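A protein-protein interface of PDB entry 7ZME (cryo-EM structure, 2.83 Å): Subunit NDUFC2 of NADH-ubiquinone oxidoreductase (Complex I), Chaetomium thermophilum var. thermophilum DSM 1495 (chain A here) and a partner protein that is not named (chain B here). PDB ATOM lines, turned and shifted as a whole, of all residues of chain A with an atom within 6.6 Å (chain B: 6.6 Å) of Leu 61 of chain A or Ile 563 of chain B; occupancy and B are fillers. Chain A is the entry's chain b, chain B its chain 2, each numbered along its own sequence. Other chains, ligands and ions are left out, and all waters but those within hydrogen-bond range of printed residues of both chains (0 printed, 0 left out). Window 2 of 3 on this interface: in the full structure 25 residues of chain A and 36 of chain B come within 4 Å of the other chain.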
ATOM      1  N   LYS A  56      10.397 -12.516 -16.819  1.00  0.00           N
ATOM      2  CA  LYS A  56       9.892 -11.293 -16.206  1.00  0.00           C
ATOM      3  C   LYS A  56      10.047 -10.096 -17.130  1.00  0.00           C
ATOM      4  O   LYS A  56       9.211  -9.189 -17.110  1.00  0.00           O
ATOM      5  CB  LYS A  56      10.601 -11.024 -14.879  1.00  0.00           C
ATOM      6  CG  LYS A  56      10.086 -11.820 -13.685  1.00  0.00           C
ATOM      7  CD  LYS A  56      10.485 -13.278 -13.727  1.00  0.00           C
ATOM      8  CE  LYS A  56      10.033 -14.011 -12.475  1.00  0.00           C
ATOM      9  NZ  LYS A  56      10.316 -15.470 -12.555  1.00  0.00           N
ATOM     10  N   GLN A  57      11.104 -10.073 -17.942  1.00  0.00           N
ATOM     11  CA  GLN A  57      11.305  -8.953 -18.852  1.00  0.00           C
ATOM     12  C   GLN A  57      10.341  -9.010 -20.025  1.00  0.00           C
ATOM     13  O   GLN A  57       9.895  -7.966 -20.512  1.00  0.00           O
ATOM     14  CB  GLN A  57      12.742  -8.936 -19.355  1.00  0.00           C
ATOM     15  CG  GLN A  57      13.739  -8.413 -18.352  1.00  0.00           C
ATOM     16  CD  GLN A  57      15.163  -8.552 -18.835  1.00  0.00           C
ATOM     17  OE1 GLN A  57      15.450  -9.320 -19.749  1.00  0.00           O
ATOM     18  NE2 GLN A  57      16.069  -7.815 -18.214  1.00  0.00           N
ATOM     19  N   THR A  58      10.019 -10.214 -20.495  1.00  0.00           N
ATOM     20  CA  THR A  58       9.045 -10.347 -21.570  1.00  0.00           C
ATOM     21  C   THR A  58       7.683  -9.825 -21.141  1.00  0.00           C
ATOM     22  O   THR A  58       7.008  -9.136 -21.911  1.00  0.00           O
ATOM     23  CB  THR A  58       8.944 -11.806 -22.005  1.00  0.00           C
ATOM     24  OG1 THR A  58      10.258 -12.365 -22.106  1.00  0.00           O
ATOM     25  CG2 THR A  58       8.244 -11.909 -23.349  1.00  0.00           C
ATOM     26  N   LYS A  59       7.266 -10.142 -19.916  1.00  0.00           N
ATOM     27  CA  LYS A  59       5.985  -9.648 -19.430  1.00  0.00           C
ATOM     28  C   LYS A  59       5.970  -8.129 -19.362  1.00  0.00           C
ATOM     29  O   LYS A  59       5.040  -7.492 -19.865  1.00  0.00           O
ATOM     30  CB  LYS A  59       5.676 -10.249 -18.061  1.00  0.00           C
ATOM     31  CG  LYS A  59       4.205 -10.200 -17.688  1.00  0.00           C
ATOM     32  CD  LYS A  59       3.989 -10.614 -16.244  1.00  0.00           C
ATOM     33  CE  LYS A  59       2.535 -10.973 -15.991  1.00  0.00           C
ATOM     34  NZ  LYS A  59       2.142 -12.216 -16.711  1.00  0.00           N
ATOM     35  N   MET A  60       7.011  -7.525 -18.785  1.00  0.00           N
ATOM     36  CA  MET A  60       7.006  -6.078 -18.587  1.00  0.00           C
ATOM     37  C   MET A  60       6.891  -5.329 -19.906  1.00  0.00           C
ATOM     38  O   MET A  60       6.189  -4.317 -19.987  1.00  0.00           O
ATOM     39  CB  MET A  60       8.254  -5.635 -17.828  1.00  0.00           C
ATOM     40  CG  MET A  60       8.306  -6.108 -16.398  1.00  0.00           C
ATOM     41  SD  MET A  60       9.791  -5.568 -15.543  1.00  0.00           S
ATOM     42  CE  MET A  60       9.562  -6.369 -13.963  1.00  0.00           C
ATOM     43  N   LEU A  61       7.571  -5.799 -20.948  1.00  0.00           N
ATOM     44  CA  LEU A  61       7.460  -5.115 -22.231  1.00  0.00           C
ATOM     45  C   LEU A  61       6.142  -5.422 -22.930  1.00  0.00           C
ATOM     46  O   LEU A  61       5.614  -4.569 -23.649  1.00  0.00           O
ATOM     47  CB  LEU A  61       8.645  -5.463 -23.128  1.00  0.00           C
ATOM     48  CG  LEU A  61       9.992  -4.949 -22.623  1.00  0.00           C
ATOM     49  CD1 LEU A  61      11.125  -5.451 -23.495  1.00  0.00           C
ATOM     50  CD2 LEU A  61       9.990  -3.435 -22.567  1.00  0.00           C
ATOM     51  N   GLU A  62       5.591  -6.623 -22.741  1.00  0.00           N
ATOM     52  CA  GLU A  62       4.273  -6.901 -23.301  1.00  0.00           C
ATOM     53  C   GLU A  62       3.195  -6.047 -22.653  1.00  0.00           C
ATOM     54  O   GLU A  62       2.321  -5.525 -23.350  1.00  0.00           O
ATOM     55  CB  GLU A  62       3.928  -8.383 -23.176  1.00  0.00           C
ATOM     56  CG  GLU A  62       4.786  -9.286 -24.043  1.00  0.00           C
ATOM     57  CD  GLU A  62       4.548  -9.063 -25.525  1.00  0.00           C
ATOM     58  OE1 GLU A  62       3.408  -8.717 -25.901  1.00  0.00           O
ATOM     59  OE2 GLU A  62       5.503  -9.229 -26.311  1.00  0.00           O
ATOM     60  N   GLU A  63       3.229  -5.896 -21.327  1.00  0.00           N
ATOM     61  CA  GLU A  63       2.333  -4.940 -20.689  1.00  0.00           C
ATOM     62  C   GLU A  63       2.639  -3.522 -21.144  1.00  0.00           C
ATOM     63  O   GLU A  63       1.727  -2.716 -21.348  1.00  0.00           O
ATOM     64  CB  GLU A  63       2.420  -5.042 -19.164  1.00  0.00           C
ATOM     65  CG  GLU A  63       2.565  -6.446 -18.620  1.00  0.00           C
ATOM     66  CD  GLU A  63       2.738  -6.468 -17.114  1.00  0.00           C
ATOM     67  OE1 GLU A  63       3.449  -5.586 -16.586  1.00  0.00           O
ATOM     68  OE2 GLU A  63       2.167  -7.365 -16.457  1.00  0.00           O
ATOM     69  N   ARG A  64       3.922  -3.197 -21.301  1.00  0.00           N
ATOM     70  CA  ARG A  64       4.288  -1.856 -21.733  1.00  0.00           C
ATOM     71  C   ARG A  64       3.839  -1.577 -23.160  1.00  0.00           C
ATOM     72  O   ARG A  64       3.293  -0.504 -23.431  1.00  0.00           O
ATOM     73  CB  ARG A  64       5.795  -1.650 -21.598  1.00  0.00           C
ATOM     74  CG  ARG A  64       6.254  -0.312 -22.105  1.00  0.00           C
ATOM     75  CD  ARG A  64       6.031   0.740 -21.047  1.00  0.00           C
ATOM     76  NE  ARG A  64       6.146   2.090 -21.579  1.00  0.00           N
ATOM     77  CZ  ARG A  64       5.114   2.893 -21.811  1.00  0.00           C
ATOM     78  NH1 ARG A  64       3.883   2.480 -21.560  1.00  0.00           N
ATOM     79  NH2 ARG A  64       5.316   4.109 -22.295  1.00  0.00           N
ATOM     80  N   LYS A  65       4.054  -2.515 -24.085  1.00  0.00           N
ATOM     81  CA  LYS A  65       3.606  -2.298 -25.457  1.00  0.00           C
ATOM     82  C   LYS A  65       2.090  -2.215 -25.543  1.00  0.00           C
ATOM     83  O   LYS A  65       1.556  -1.459 -26.360  1.00  0.00           O
ATOM     84  CB  LYS A  65       4.129  -3.393 -26.389  1.00  0.00           C
ATOM     85  CG  LYS A  65       5.642  -3.433 -26.539  1.00  0.00           C
ATOM     86  CD  LYS A  65       6.065  -4.497 -27.537  1.00  0.00           C
ATOM     87  CE  LYS A  65       5.852  -5.908 -27.012  1.00  0.00           C
ATOM     88  NZ  LYS A  65       6.734  -6.215 -25.856  1.00  0.00           N
ATOM     89  N   GLN A  66       1.382  -2.984 -24.717  1.00  0.00           N
ATOM     90  CA  GLN A  66      -0.064  -2.828 -24.634  1.00  0.00           C
ATOM     91  C   GLN A  66      -0.434  -1.460 -24.075  1.00  0.00           C
ATOM     92  O   GLN A  66      -1.382  -0.824 -24.547  1.00  0.00           O
ATOM     93  CB  GLN A  66      -0.664  -3.942 -23.780  1.00  0.00           C
ATOM     94  CG  GLN A  66      -0.658  -5.301 -24.450  1.00  0.00           C
ATOM     95  CD  GLN A  66      -0.841  -5.216 -25.952  1.00  0.00           C
ATOM     96  OE1 GLN A  66       0.045  -5.594 -26.718  1.00  0.00           O
ATOM     97  NE2 GLN A  66      -2.004  -4.738 -26.383  1.00  0.00           N
ATOM     98  N   ALA A  67       0.309  -0.993 -23.070  1.00  0.00           N
ATOM     99  CA  ALA A  67       0.039   0.315 -22.487  1.00  0.00           C
ATOM    100  C   ALA A  67       0.249   1.433 -23.499  1.00  0.00           C
ATOM    101  O   ALA A  67      -0.502   2.414 -23.513  1.00  0.00           O
ATOM    102  CB  ALA A  67       0.919   0.530 -21.258  1.00  0.00           C
ATOM    103  N   ILE B  47       6.958  -0.681  -9.519  1.00  0.00           N
ATOM    104  CA  ILE B  47       7.236   0.095 -10.760  1.00  0.00           C
ATOM    105  C   ILE B  47       6.897   1.552 -10.444  1.00  0.00           C
ATOM    106  O   ILE B  47       5.773   1.796  -9.975  1.00  0.00           O
ATOM    107  CB  ILE B  47       6.456  -0.450 -11.967  1.00  0.00           C
ATOM    108  CG1 ILE B  47       6.811  -1.906 -12.274  1.00  0.00           C
ATOM    109  CG2 ILE B  47       6.661   0.441 -13.183  1.00  0.00           C
ATOM    110  CD1 ILE B  47       8.195  -2.088 -12.841  1.00  0.00           C
ATOM    111  N   GLN B 364      18.700   4.574 -23.248  1.00  0.00           N
ATOM    112  CA  GLN B 364      19.170   3.193 -23.275  1.00  0.00           C
ATOM    113  C   GLN B 364      20.646   3.132 -23.638  1.00  0.00           C
ATOM    114  O   GLN B 364      21.405   2.351 -23.055  1.00  0.00           O
ATOM    115  CB  GLN B 364      18.352   2.369 -24.266  1.00  0.00           C
ATOM    116  CG  GLN B 364      16.870   2.394 -24.027  1.00  0.00           C
ATOM    117  CD  GLN B 364      16.088   1.819 -25.182  1.00  0.00           C
ATOM    118  OE1 GLN B 364      16.611   1.649 -26.278  1.00  0.00           O
ATOM    119  NE2 GLN B 364      14.822   1.515 -24.941  1.00  0.00           N
ATOM    120  N   LEU B 558      20.448  -5.930 -22.261  1.00  0.00           N
ATOM    121  CA  LEU B 558      19.943  -4.809 -23.076  1.00  0.00           C
ATOM    122  C   LEU B 558      18.479  -4.588 -22.720  1.00  0.00           C
ATOM    123  O   LEU B 558      18.028  -3.443 -22.807  1.00  0.00           O
ATOM    124  CB  LEU B 558      20.156  -5.126 -24.560  1.00  0.00           C
ATOM    125  CG  LEU B 558      21.566  -4.876 -25.085  1.00  0.00           C
ATOM    126  CD1 LEU B 558      21.680  -5.301 -26.536  1.00  0.00           C
ATOM    127  CD2 LEU B 558      21.944  -3.415 -24.929  1.00  0.00           C
ATOM    128  N   SER B 559      17.780  -5.657 -22.323  1.00  0.00           N
ATOM    129  CA  SER B 559      16.367  -5.503 -22.003  1.00  0.00           C
ATOM    130  C   SER B 559      16.166  -4.824 -20.657  1.00  0.00           C
ATOM    131  O   SER B 559      15.122  -4.208 -20.427  1.00  0.00           O
ATOM    132  CB  SER B 559      15.675  -6.859 -22.023  1.00  0.00           C
ATOM    133  OG  SER B 559      16.073  -7.610 -23.154  1.00  0.00           O
ATOM    134  N   MET B 560      17.148  -4.928 -19.759  1.00  0.00           N
ATOM    135  CA  MET B 560      17.077  -4.188 -18.506  1.00  0.00           C
ATOM    136  C   MET B 560      17.021  -2.689 -18.762  1.00  0.00           C
ATOM    137  O   MET B 560      16.221  -1.976 -18.146  1.00  0.00           O
ATOM    138  CB  MET B 560      18.278  -4.521 -17.628  1.00  0.00           C
ATOM    139  CG  MET B 560      18.243  -3.826 -16.279  1.00  0.00           C
ATOM    140  SD  MET B 560      19.656  -4.239 -15.250  1.00  0.00           S
ATOM    141  CE  MET B 560      20.938  -3.341 -16.117  1.00  0.00           C
ATOM    142  N   GLY B 561      17.866  -2.194 -19.666  1.00  0.00           N
ATOM    143  CA  GLY B 561      17.869  -0.778 -19.966  1.00  0.00           C
ATOM    144  C   GLY B 561      16.673  -0.327 -20.769  1.00  0.00           C
ATOM    145  O   GLY B 561      16.267   0.833 -20.674  1.00  0.00           O
ATOM    146  N   THR B 562      16.097  -1.220 -21.573  1.00  0.00           N
ATOM    147  CA  THR B 562      14.864  -0.883 -22.274  1.00  0.00           C
ATOM    148  C   THR B 562      13.735  -0.614 -21.291  1.00  0.00           C
ATOM    149  O   THR B 562      12.991   0.360 -21.439  1.00  0.00           O
ATOM    150  CB  THR B 562      14.478  -2.013 -23.228  1.00  0.00           C
ATOM    151  OG1 THR B 562      15.644  -2.478 -23.914  1.00  0.00           O
ATOM    152  CG2 THR B 562      13.463  -1.528 -24.244  1.00  0.00           C
ATOM    153  N   ILE B 563      13.621  -1.419 -20.242  1.00  0.00           N
ATOM    154  CA  ILE B 563      12.515  -1.266 -19.262  1.00  0.00           C
ATOM    155  C   ILE B 563      12.763  -0.033 -18.392  1.00  0.00           C
ATOM    156  O   ILE B 563      11.813   0.722 -18.173  1.00  0.00           O
ATOM    157  CB  ILE B 563      12.335  -2.556 -18.439  1.00  0.00           C
ATOM    158  CG1 ILE B 563      11.982  -3.741 -19.341  1.00  0.00           C
ATOM    159  CG2 ILE B 563      11.312  -2.378 -17.331  1.00  0.00           C
ATOM    160  CD1 ILE B 563      11.998  -5.072 -18.644  1.00  0.00           C
ATOM    161  N   LEU B 564      13.994   0.179 -17.935  1.00  0.00           N
ATOM    162  CA  LEU B 564      14.269   1.289 -17.002  1.00  0.00           C
ATOM    163  C   LEU B 564      13.929   2.590 -17.709  1.00  0.00           C
ATOM    164  O   LEU B 564      13.348   3.470 -17.067  1.00  0.00           O
ATOM    165  CB  LEU B 564      15.747   1.231 -16.623  1.00  0.00           C
ATOM    166  CG  LEU B 564      16.060   1.003 -15.148  1.00  0.00           C
ATOM    167  CD1 LEU B 564      14.945   0.233 -14.467  1.00  0.00           C
ATOM    168  CD2 LEU B 564      17.389   0.284 -14.993  1.00  0.00           C
ATOM    169  N   VAL B 565      14.285   2.691 -18.985  1.00  0.00           N
ATOM    170  CA  VAL B 565      14.053   3.934 -19.769  1.00  0.00           C
ATOM    171  C   VAL B 565      12.567   4.085 -20.076  1.00  0.00           C
ATOM    172  O   VAL B 565      12.084   5.213 -20.040  1.00  0.00           O
ATOM    173  CB  VAL B 565      14.926   3.935 -21.034  1.00  0.00           C
ATOM    174  CG1 VAL B 565      14.611   5.098 -21.956  1.00  0.00           C
ATOM    175  CG2 VAL B 565      16.395   3.931 -20.657  1.00  0.00           C
ATOM    176  N   GLN B 566      11.869   2.983 -20.318  1.00  0.00           N
ATOM    177  CA  GLN B 566      10.432   3.078 -20.551  1.00  0.00           C
ATOM    178  C   GLN B 566       9.715   3.619 -19.324  1.00  0.00           C
ATOM    179  O   GLN B 566       8.774   4.408 -19.447  1.00  0.00           O
ATOM    180  CB  GLN B 566       9.856   1.719 -20.952  1.00  0.00           C
ATOM    181  CG  GLN B 566      10.177   1.297 -22.381  1.00  0.00           C
ATOM    182  CD  GLN B 566       9.587   2.221 -23.420  1.00  0.00           C
ATOM    183  OE1 GLN B 566       8.378   2.434 -23.464  1.00  0.00           O
ATOM    184  NE2 GLN B 566      10.437   2.785 -24.257  1.00  0.00           N
ATOM    185  N   ILE B 567      10.147   3.209 -18.130  1.00  0.00           N
ATOM    186  CA  ILE B 567       9.553   3.724 -16.898  1.00  0.00           C
ATOM    187  C   ILE B 567       9.833   5.215 -16.752  1.00  0.00           C
ATOM    188  O   ILE B 567       8.949   5.997 -16.385  1.00  0.00           O
ATOM    189  CB  ILE B 567      10.063   2.930 -15.683  1.00  0.00           C
ATOM    190  CG1 ILE B 567       9.618   1.470 -15.778  1.00  0.00           C
ATOM    191  CG2 ILE B 567       9.586   3.562 -14.384  1.00  0.00           C
ATOM    192  CD1 ILE B 567      10.352   0.543 -14.846  1.00  0.00           C
ATOM    193  N   LEU B 568      11.068   5.631 -17.037  1.00  0.00           N
ATOM    194  CA  LEU B 568      11.435   7.036 -16.883  1.00  0.00           C
ATOM    195  C   LEU B 568      10.666   7.936 -17.843  1.00  0.00           C
ATOM    196  O   LEU B 568      10.412   9.102 -17.525  1.00  0.00           O
ATOM    197  CB  LEU B 568      12.942   7.205 -17.083  1.00  0.00           C
ATOM    198  CG  LEU B 568      13.510   8.629 -17.154  1.00  0.00           C
ATOM    199  CD1 LEU B 568      13.507   9.308 -15.797  1.00  0.00           C
ATOM    200  CD2 LEU B 568      14.901   8.625 -17.751  1.00  0.00           C
ATOM    201  N   SER B 570       7.571   7.093 -19.157  1.00  0.00           N
ATOM    202  CA  SER B 570       6.177   6.688 -19.211  1.00  0.00           C
ATOM    203  C   SER B 570       5.276   7.706 -18.516  1.00  0.00           C
ATOM    204  O   SER B 570       5.704   8.790 -18.116  1.00  0.00           O
ATOM    205  CB  SER B 570       5.998   5.309 -18.583  1.00  0.00           C
ATOM    206  OG  SER B 570       6.501   4.300 -19.437  1.00  0.00           O
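Of chain B, only Ile 563 (3.8 Å) comes within 4 Å of Leu 61 of chain A.
Printed residues of chain A within 4 Å of Ile 563 of chain B: Gln 57 (3.8 Å), Met 60 (3.8 Å) and Leu 61 (3.8 Å).
Printed residues of chain A within 4 Å of Gln 566 of chain B: Arg 64.
Of the printed residues of chain A, Ser 570 of chain B touches Arg 64.
Gln 57 of chain A touches Ser 559 of chain B.
Ile 563 of chain B touches Gln 57 of chain A (CD1 to CG, 3.8 Å).
Ile 563 of chain B touches Met 60 of chain A.
Leu 61 of chain A touches Ile 563 of chain B.
O of Leu 61 of chain A sits at hydrogen-bond distance from NZ of Lys 65 of chain A.
The backbone NH (N) of Met 560 of chain B sits close to the side-chain amide nitrogen (NE2) of Gln 57 of chain A (3.4 Å).
OE1 of Gln 566 of chain B is in hydrogen-bond range of NE of Arg 64 of chain A (2.9 Å).
The guanidinium group (NE) of Arg 64 of chain A lies close to the side-chain hydroxyl (OG) of Ser 570 of chain B (3.1 Å).
Hydrophobic or aromatic side chains of chain A within 4 Å of the printed part of chain B: Met 60 and Leu 61.
Along chain A the printed residues that touch a printed residue of chain B span positions 57 to 64.
Of the 14 printed residues of chain B, 5 touch a printed residue of chain A.
Hydrophobic or aromatic side chains of chain B within 4 Å of the printed part of chain A: Ile 563.
Among the printed residues, 7 pairs touch across the chains.
Among the printed residues, no Asp or Glu carboxylate lies within 4 Å of a Lys or Arg side-chain nitrogen of the other chain.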
